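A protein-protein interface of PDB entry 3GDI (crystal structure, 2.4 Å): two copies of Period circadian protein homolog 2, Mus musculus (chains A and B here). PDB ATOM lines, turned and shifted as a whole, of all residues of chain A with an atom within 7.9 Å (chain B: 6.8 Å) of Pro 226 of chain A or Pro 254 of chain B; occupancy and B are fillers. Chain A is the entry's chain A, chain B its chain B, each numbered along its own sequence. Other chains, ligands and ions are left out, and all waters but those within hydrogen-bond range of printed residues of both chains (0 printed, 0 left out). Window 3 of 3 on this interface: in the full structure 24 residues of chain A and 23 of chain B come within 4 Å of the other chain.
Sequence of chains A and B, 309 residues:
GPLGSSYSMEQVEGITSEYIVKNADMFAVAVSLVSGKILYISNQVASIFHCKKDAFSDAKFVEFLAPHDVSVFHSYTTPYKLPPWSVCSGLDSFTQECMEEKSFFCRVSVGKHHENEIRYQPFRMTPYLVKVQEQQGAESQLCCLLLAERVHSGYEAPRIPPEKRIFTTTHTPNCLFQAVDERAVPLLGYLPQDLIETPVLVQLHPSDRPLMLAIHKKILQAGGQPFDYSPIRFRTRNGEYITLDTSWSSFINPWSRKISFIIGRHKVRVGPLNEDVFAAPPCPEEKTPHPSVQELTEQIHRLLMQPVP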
ATOM      1  N   ILE A 219     -30.709   6.059 -26.651  1.00  0.00           N
ATOM      2  CA  ILE A 219     -29.307   6.235 -27.013  1.00  0.00           C
ATOM      3  C   ILE A 219     -28.815   5.233 -28.045  1.00  0.00           C
ATOM      4  O   ILE A 219     -28.198   5.619 -29.031  1.00  0.00           O
ATOM      5  CB  ILE A 219     -28.377   6.149 -25.784  1.00  0.00           C
ATOM      6  CG1 ILE A 219     -28.575   7.376 -24.892  1.00  0.00           C
ATOM      7  CG2 ILE A 219     -26.931   6.054 -26.232  1.00  0.00           C
ATOM      8  CD1 ILE A 219     -27.713   7.360 -23.647  1.00  0.00           C
ATOM      9  N   ALA A 222     -30.674   5.856 -31.201  1.00  0.00           N
ATOM     10  CA  ALA A 222     -30.193   7.032 -31.914  1.00  0.00           C
ATOM     11  C   ALA A 222     -28.886   6.746 -32.643  1.00  0.00           C
ATOM     12  O   ALA A 222     -28.398   7.579 -33.412  1.00  0.00           O
ATOM     13  CB  ALA A 222     -30.003   8.187 -30.939  1.00  0.00           C
ATOM     14  N   GLY A 223     -28.318   5.572 -32.380  1.00  0.00           N
ATOM     15  CA  GLY A 223     -27.075   5.172 -33.016  1.00  0.00           C
ATOM     16  C   GLY A 223     -25.941   6.184 -33.047  1.00  0.00           C
ATOM     17  O   GLY A 223     -25.118   6.154 -33.962  1.00  0.00           O
ATOM     18  N   GLY A 224     -25.877   7.079 -32.066  1.00  0.00           N
ATOM     19  CA  GLY A 224     -24.793   8.051 -32.052  1.00  0.00           C
ATOM     20  C   GLY A 224     -25.206   9.505 -32.206  1.00  0.00           C
ATOM     21  O   GLY A 224     -24.464  10.403 -31.807  1.00  0.00           O
ATOM     22  N   GLN A 225     -26.376   9.747 -32.787  1.00  0.00           N
ATOM     23  CA  GLN A 225     -26.865  11.109 -32.968  1.00  0.00           C
ATOM     24  C   GLN A 225     -27.315  11.646 -31.605  1.00  0.00           C
ATOM     25  O   GLN A 225     -28.230  11.105 -30.983  1.00  0.00           O
ATOM     26  CB  GLN A 225     -28.040  11.104 -33.960  1.00  0.00           C
ATOM     27  CG  GLN A 225     -28.598  12.482 -34.348  1.00  0.00           C
ATOM     28  CD  GLN A 225     -27.607  13.338 -35.136  1.00  0.00           C
ATOM     29  OE1 GLN A 225     -27.059  12.907 -36.155  1.00  0.00           O
ATOM     30  NE2 GLN A 225     -27.382  14.561 -34.670  1.00  0.00           N
ATOM     31  N   PRO A 226     -26.675  12.718 -31.120  1.00  0.00           N
ATOM     32  CA  PRO A 226     -27.036  13.303 -29.819  1.00  0.00           C
ATOM     33  C   PRO A 226     -28.510  13.710 -29.713  1.00  0.00           C
ATOM     34  O   PRO A 226     -29.138  14.050 -30.712  1.00  0.00           O
ATOM     35  CB  PRO A 226     -26.108  14.514 -29.711  1.00  0.00           C
ATOM     36  CG  PRO A 226     -24.923  14.122 -30.546  1.00  0.00           C
ATOM     37  CD  PRO A 226     -25.557  13.452 -31.737  1.00  0.00           C
ATOM     38  N   PHE A 227     -29.059  13.671 -28.504  1.00  0.00           N
ATOM     39  CA  PHE A 227     -30.442  14.080 -28.298  1.00  0.00           C
ATOM     40  C   PHE A 227     -30.618  14.631 -26.888  1.00  0.00           C
ATOM     41  O   PHE A 227     -29.935  14.213 -25.956  1.00  0.00           O
ATOM     42  CB  PHE A 227     -31.408  12.911 -28.552  1.00  0.00           C
ATOM     43  CG  PHE A 227     -31.441  11.880 -27.458  1.00  0.00           C
ATOM     44  CD1 PHE A 227     -32.165  12.107 -26.285  1.00  0.00           C
ATOM     45  CD2 PHE A 227     -30.789  10.653 -27.623  1.00  0.00           C
ATOM     46  CE1 PHE A 227     -32.245  11.123 -25.292  1.00  0.00           C
ATOM     47  CE2 PHE A 227     -30.865   9.664 -26.639  1.00  0.00           C
ATOM     48  CZ  PHE A 227     -31.596   9.897 -25.469  1.00  0.00           C
ATOM     49  N   ASP A 228     -31.544  15.574 -26.740  1.00  0.00           N
ATOM     50  CA  ASP A 228     -31.794  16.201 -25.453  1.00  0.00           C
ATOM     51  C   ASP A 228     -32.833  15.525 -24.581  1.00  0.00           C
ATOM     52  O   ASP A 228     -33.786  14.906 -25.058  1.00  0.00           O
ATOM     53  CB  ASP A 228     -32.210  17.651 -25.657  1.00  0.00           C
ATOM     54  CG  ASP A 228     -31.128  18.479 -26.307  1.00  0.00           C
ATOM     55  OD1 ASP A 228     -31.446  19.575 -26.813  1.00  0.00           O
ATOM     56  OD2 ASP A 228     -29.961  18.040 -26.305  1.00  0.00           O
ATOM     57  N   TYR A 229     -32.619  15.655 -23.280  1.00  0.00           N
ATOM     58  CA  TYR A 229     -33.530  15.130 -22.294  1.00  0.00           C
ATOM     59  C   TYR A 229     -33.339  15.951 -21.039  1.00  0.00           C
ATOM     60  O   TYR A 229     -32.215  16.192 -20.607  1.00  0.00           O
ATOM     61  CB  TYR A 229     -33.258  13.661 -21.980  1.00  0.00           C
ATOM     62  CG  TYR A 229     -34.304  13.089 -21.052  1.00  0.00           C
ATOM     63  CD1 TYR A 229     -35.398  12.381 -21.550  1.00  0.00           C
ATOM     64  CD2 TYR A 229     -34.251  13.337 -19.678  1.00  0.00           C
ATOM     65  CE1 TYR A 229     -36.419  11.938 -20.699  1.00  0.00           C
ATOM     66  CE2 TYR A 229     -35.264  12.904 -18.821  1.00  0.00           C
ATOM     67  CZ  TYR A 229     -36.344  12.207 -19.336  1.00  0.00           C
ATOM     68  OH  TYR A 229     -37.348  11.796 -18.483  1.00  0.00           O
ATOM     69  N   THR A 246     -29.754  17.721 -20.176  1.00  0.00           N
ATOM     70  CA  THR A 246     -28.735  16.875 -20.754  1.00  0.00           C
ATOM     71  C   THR A 246     -28.883  16.489 -22.200  1.00  0.00           C
ATOM     72  O   THR A 246     -29.984  16.359 -22.722  1.00  0.00           O
ATOM     73  CB  THR A 246     -28.607  15.579 -19.940  1.00  0.00           C
ATOM     74  OG1 THR A 246     -28.328  15.901 -18.569  1.00  0.00           O
ATOM     75  CG2 THR A 246     -27.494  14.710 -20.495  1.00  0.00           C
ATOM     76  N   SER A 247     -27.736  16.305 -22.834  1.00  0.00           N
ATOM     77  CA  SER A 247     -27.660  15.873 -24.217  1.00  0.00           C
ATOM     78  C   SER A 247     -26.913  14.537 -24.144  1.00  0.00           C
ATOM     79  O   SER A 247     -25.818  14.466 -23.598  1.00  0.00           O
ATOM     80  CB  SER A 247     -26.872  16.881 -25.042  1.00  0.00           C
ATOM     81  OG  SER A 247     -26.403  16.279 -26.236  1.00  0.00           O
ATOM     82  N   TRP A 248     -27.513  13.481 -24.677  1.00  0.00           N
ATOM     83  CA  TRP A 248     -26.897  12.164 -24.623  1.00  0.00           C
ATOM     84  C   TRP A 248     -26.379  11.627 -25.956  1.00  0.00           C
ATOM     85  O   TRP A 248     -26.983  11.843 -27.006  1.00  0.00           O
ATOM     86  CB  TRP A 248     -27.877  11.148 -24.038  1.00  0.00           C
ATOM     87  CG  TRP A 248     -28.259  11.411 -22.615  1.00  0.00           C
ATOM     88  CD1 TRP A 248     -29.418  11.981 -22.168  1.00  0.00           C
ATOM     89  CD2 TRP A 248     -27.461  11.144 -21.444  1.00  0.00           C
ATOM     90  NE1 TRP A 248     -29.392  12.086 -20.793  1.00  0.00           N
ATOM     91  CE2 TRP A 248     -28.201  11.584 -20.325  1.00  0.00           C
ATOM     92  CE3 TRP A 248     -26.189  10.581 -21.237  1.00  0.00           C
ATOM     93  CZ2 TRP A 248     -27.713  11.484 -19.018  1.00  0.00           C
ATOM     94  CZ3 TRP A 248     -25.703  10.483 -19.942  1.00  0.00           C
ATOM     95  CH2 TRP A 248     -26.466  10.935 -18.847  1.00  0.00           C
ATOM     96  N   SER A 249     -25.255  10.911 -25.894  1.00  0.00           N
ATOM     97  CA  SER A 249     -24.648  10.320 -27.079  1.00  0.00           C
ATOM     98  C   SER A 249     -23.848   9.059 -26.716  1.00  0.00           C
ATOM     99  O   SER A 249     -23.706   8.713 -25.539  1.00  0.00           O
ATOM    100  CB  SER A 249     -23.740  11.338 -27.762  1.00  0.00           C
ATOM    101  OG  SER A 249     -23.428  10.915 -29.079  1.00  0.00           O
ATOM    102  N   SER A 250     -23.328   8.362 -27.721  1.00  0.00           N
ATOM    103  CA  SER A 250     -22.559   7.156 -27.447  1.00  0.00           C
ATOM    104  C   SER A 250     -21.419   6.980 -28.423  1.00  0.00           C
ATOM    105  O   SER A 250     -21.446   7.523 -29.523  1.00  0.00           O
ATOM    106  CB  SER A 250     -23.460   5.922 -27.531  1.00  0.00           C
ATOM    107  OG  SER A 250     -24.118   5.874 -28.781  1.00  0.00           O
ATOM    108  N   PHE A 251     -20.402   6.238 -28.000  1.00  0.00           N
ATOM    109  CA  PHE A 251     -19.289   5.932 -28.874  1.00  0.00           C
ATOM    110  C   PHE A 251     -19.517   4.469 -29.249  1.00  0.00           C
ATOM    111  O   PHE A 251     -19.599   3.610 -28.375  1.00  0.00           O
ATOM    112  CB  PHE A 251     -17.949   6.114 -28.156  1.00  0.00           C
ATOM    113  CG  PHE A 251     -17.592   7.558 -27.885  1.00  0.00           C
ATOM    114  CD1 PHE A 251     -17.891   8.553 -28.818  1.00  0.00           C
ATOM    115  CD2 PHE A 251     -16.931   7.920 -26.715  1.00  0.00           C
ATOM    116  CE1 PHE A 251     -17.529   9.891 -28.592  1.00  0.00           C
ATOM    117  CE2 PHE A 251     -16.567   9.246 -26.476  1.00  0.00           C
ATOM    118  CZ  PHE A 251     -16.866  10.236 -27.418  1.00  0.00           C
ATOM    119  N   ILE A 263     -21.771   9.035 -23.473  1.00  0.00           N
ATOM    120  CA  ILE A 263     -21.289  10.358 -23.082  1.00  0.00           C
ATOM    121  C   ILE A 263     -22.417  11.347 -22.922  1.00  0.00           C
ATOM    122  O   ILE A 263     -23.322  11.402 -23.751  1.00  0.00           O
ATOM    123  CB  ILE A 263     -20.327  10.946 -24.100  1.00  0.00           C
ATOM    124  CG1 ILE A 263     -20.878  10.733 -25.507  1.00  0.00           C
ATOM    125  CG2 ILE A 263     -18.968  10.335 -23.928  1.00  0.00           C
ATOM    126  CD1 ILE A 263     -19.955  11.214 -26.612  1.00  0.00           C
ATOM    127  N   GLY A 264     -22.356  12.138 -21.858  1.00  0.00           N
ATOM    128  CA  GLY A 264     -23.386  13.125 -21.618  1.00  0.00           C
ATOM    129  C   GLY A 264     -22.783  14.505 -21.449  1.00  0.00           C
ATOM    130  O   GLY A 264     -21.718  14.665 -20.858  1.00  0.00           O
ATOM    131  N   ARG A 265     -23.459  15.511 -21.990  1.00  0.00           N
ATOM    132  CA  ARG A 265     -22.999  16.886 -21.879  1.00  0.00           C
ATOM    133  C   ARG A 265     -24.083  17.577 -21.096  1.00  0.00           C
ATOM    134  O   ARG A 265     -25.181  17.777 -21.601  1.00  0.00           O
ATOM    135  CB  ARG A 265     -22.870  17.531 -23.250  1.00  0.00           C
ATOM    136  CG  ARG A 265     -22.294  18.923 -23.174  1.00  0.00           C
ATOM    137  CD  ARG A 265     -22.235  19.553 -24.517  1.00  0.00           C
ATOM    138  NE  ARG A 265     -21.216  20.590 -24.569  1.00  0.00           N
ATOM    139  CZ  ARG A 265     -21.465  21.886 -24.438  1.00  0.00           C
ATOM    140  NH1 ARG A 265     -22.712  22.301 -24.242  1.00  0.00           N
ATOM    141  NH2 ARG A 265     -20.467  22.762 -24.515  1.00  0.00           N
ATOM    142  N   ILE B 252     -14.839  10.547 -31.483  1.00  0.00           N
ATOM    143  CA  ILE B 252     -14.837  12.001 -31.487  1.00  0.00           C
ATOM    144  C   ILE B 252     -15.954  12.582 -30.631  1.00  0.00           C
ATOM    145  O   ILE B 252     -17.126  12.297 -30.876  1.00  0.00           O
ATOM    146  CB  ILE B 252     -15.023  12.510 -32.945  1.00  0.00           C
ATOM    147  CG1 ILE B 252     -13.889  11.992 -33.831  1.00  0.00           C
ATOM    148  CG2 ILE B 252     -15.076  14.014 -32.986  1.00  0.00           C
ATOM    149  CD1 ILE B 252     -14.135  12.199 -35.327  1.00  0.00           C
ATOM    150  N   ASN B 253     -15.608  13.383 -29.629  1.00  0.00           N
ATOM    151  CA  ASN B 253     -16.639  14.017 -28.812  1.00  0.00           C
ATOM    152  C   ASN B 253     -17.507  14.819 -29.811  1.00  0.00           C
ATOM    153  O   ASN B 253     -16.992  15.635 -30.575  1.00  0.00           O
ATOM    154  CB  ASN B 253     -15.991  14.951 -27.790  1.00  0.00           C
ATOM    155  CG  ASN B 253     -17.003  15.634 -26.896  1.00  0.00           C
ATOM    156  OD1 ASN B 253     -17.884  16.358 -27.365  1.00  0.00           O
ATOM    157  ND2 ASN B 253     -16.876  15.413 -25.592  1.00  0.00           N
ATOM    158  N   PRO B 254     -18.830  14.597 -29.810  1.00  0.00           N
ATOM    159  CA  PRO B 254     -19.765  15.279 -30.715  1.00  0.00           C
ATOM    160  C   PRO B 254     -19.987  16.777 -30.521  1.00  0.00           C
ATOM    161  O   PRO B 254     -20.560  17.436 -31.389  1.00  0.00           O
ATOM    162  CB  PRO B 254     -21.077  14.511 -30.517  1.00  0.00           C
ATOM    163  CG  PRO B 254     -20.675  13.230 -29.842  1.00  0.00           C
ATOM    164  CD  PRO B 254     -19.551  13.643 -28.953  1.00  0.00           C
ATOM    165  N   TRP B 255     -19.535  17.321 -29.398  1.00  0.00           N
ATOM    166  CA  TRP B 255     -19.766  18.728 -29.117  1.00  0.00           C
ATOM    167  C   TRP B 255     -18.539  19.581 -29.320  1.00  0.00           C
ATOM    168  O   TRP B 255     -18.629  20.669 -29.867  1.00  0.00           O
ATOM    169  CB  TRP B 255     -20.300  18.871 -27.685  1.00  0.00           C
ATOM    170  CG  TRP B 255     -21.553  18.043 -27.452  1.00  0.00           C
ATOM    171  CD1 TRP B 255     -22.802  18.293 -27.939  1.00  0.00           C
ATOM    172  CD2 TRP B 255     -21.643  16.784 -26.760  1.00  0.00           C
ATOM    173  NE1 TRP B 255     -23.661  17.266 -27.603  1.00  0.00           N
ATOM    174  CE2 TRP B 255     -22.973  16.331 -26.882  1.00  0.00           C
ATOM    175  CE3 TRP B 255     -20.726  15.994 -26.056  1.00  0.00           C
ATOM    176  CZ2 TRP B 255     -23.408  15.130 -26.329  1.00  0.00           C
ATOM    177  CZ3 TRP B 255     -21.166  14.793 -25.506  1.00  0.00           C
ATOM    178  CH2 TRP B 255     -22.491  14.376 -25.648  1.00  0.00           C
ATOM    179  N   SER B 256     -17.388  19.089 -28.886  1.00  0.00           N
ATOM    180  CA  SER B 256     -16.152  19.837 -29.040  1.00  0.00           C
ATOM    181  C   SER B 256     -15.394  19.386 -30.296  1.00  0.00           C
ATOM    182  O   SER B 256     -14.404  20.001 -30.707  1.00  0.00           O
ATOM    183  CB  SER B 256     -15.277  19.644 -27.801  1.00  0.00           C
ATOM    184  OG  SER B 256     -14.928  18.284 -27.632  1.00  0.00           O
ATOM    185  N   ARG B 257     -15.872  18.305 -30.899  1.00  0.00           N
ATOM    186  CA  ARG B 257     -15.264  17.740 -32.099  1.00  0.00           C
ATOM    187  C   ARG B 257     -13.840  17.253 -31.909  1.00  0.00           C
ATOM    188  O   ARG B 257     -13.126  17.063 -32.878  1.00  0.00           O
ATOM    189  CB  ARG B 257     -15.297  18.742 -33.256  1.00  0.00           C
ATOM    190  CG  ARG B 257     -16.694  19.089 -33.743  1.00  0.00           C
ATOM    191  CD  ARG B 257     -17.526  17.832 -33.980  1.00  0.00           C
ATOM    192  NE  ARG B 257     -16.905  16.910 -34.931  1.00  0.00           N
ATOM    193  CZ  ARG B 257     -17.388  15.702 -35.223  1.00  0.00           C
ATOM    194  NH1 ARG B 257     -18.500  15.270 -34.644  1.00  0.00           N
ATOM    195  NH2 ARG B 257     -16.754  14.917 -36.084  1.00  0.00           N
ATOM    196  N   LYS B 258     -13.422  17.052 -30.665  1.00  0.00           N
ATOM    197  CA  LYS B 258     -12.071  16.557 -30.403  1.00  0.00           C
ATOM    198  C   LYS B 258     -12.102  15.054 -30.141  1.00  0.00           C
ATOM    199  O   LYS B 258     -13.107  14.513 -29.680  1.00  0.00           O
ATOM    200  CB  LYS B 258     -11.448  17.266 -29.195  1.00  0.00           C
ATOM    201  CG  LYS B 258     -11.324  18.764 -29.357  1.00  0.00           C
ATOM    202  CD  LYS B 258     -10.287  19.339 -28.411  1.00  0.00           C
ATOM    203  CE  LYS B 258     -10.534  18.921 -26.958  1.00  0.00           C
ATOM    204  NZ  LYS B 258     -11.850  19.411 -26.432  1.00  0.00           N
ATOM    205  N   SER B 260     -11.610  11.744 -28.228  1.00  0.00           N
ATOM    206  CA  SER B 260     -11.590  11.340 -26.831  1.00  0.00           C
ATOM    207  C   SER B 260     -10.838  10.013 -26.691  1.00  0.00           C
ATOM    208  O   SER B 260     -10.127   9.797 -25.711  1.00  0.00           O
ATOM    209  CB  SER B 260     -13.016  11.167 -26.321  1.00  0.00           C
ATOM    210  OG  SER B 260     -13.806  12.309 -26.587  1.00  0.00           O
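Among the printed residues, merely in contact across the chains: Phe 251 of chain A with Ile 252 of chain B, Arg 265 of chain A with Trp 255 of chain B, Ile 263 of chain A with Pro 254 of chain B, Ile 263 of chain A with Trp 255 of chain B, Ser 249 of chain A with Pro 254 of chain B, Phe 251 of chain A with Ser 260 of chain B, Pro 226 of chain A with Pro 254 of chain B and Ser 249 of chain A with Trp 255 of chain B.
Of chain A, only Pro 226 (3.9 Å), Ser 249 (3.7 Å) and Ile 263 (3.4 Å) come within 4 Å of Pro 254 of chain B.
Of the printed residues of chain A, Trp 255 of chain B touches Ser 247 (3.2 Å), Ser 249 (3.9 Å), Ile 263 (3.6 Å) and Arg 265 (3.4 Å).
Of the printed residues of chain B, Phe 251 of chain A touches Ile 252 and Ser 260.
Asn 253 of chain B touches none of the printed residues of chain A.
Lys 258 of chain B touches none of the printed residues of chain A.
The nearest residue of chain A that does not touch Pro 254 of chain B is Phe 251 of chain A (4.3 Å).
The side-chain hydroxyl (OG) of Ser 247 of chain A lies close to the indole nitrogen (NE1) of Trp 255 of chain B (3.2 Å).
Hydrophobic or aromatic side chains of chain B within 4 Å of the printed part of chain A: Pro 254 and Trp 255.
Hydrophobic or aromatic side chains of chain A within 4 Å of the printed part of chain B: Pro 226, Phe 251 and Ile 263.
Among the printed residues, 9 pairs touch across the chains.
N of Arg 265 of chain A sits at hydrogen-bond distance from O of Ser 247 of chain A.
The side-chain hydroxyl of Ser 249 of chain A lies within hydrogen-bond range of the backbone carbonyl oxygen of Gly 224 of chain A (3.0 Å).
The backbone carbonyl oxygen (O) of Ser 249 of chain A is in hydrogen-bond range of the backbone NH (N) of Ile 263 of chain A (2.8 Å).
The side-chain amide oxygen (OD1) of Asn 253 of chain B is in hydrogen-bond range of the backbone NH (N) of Trp 255 of chain B (2.8 Å).
No position is printed for both chains.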
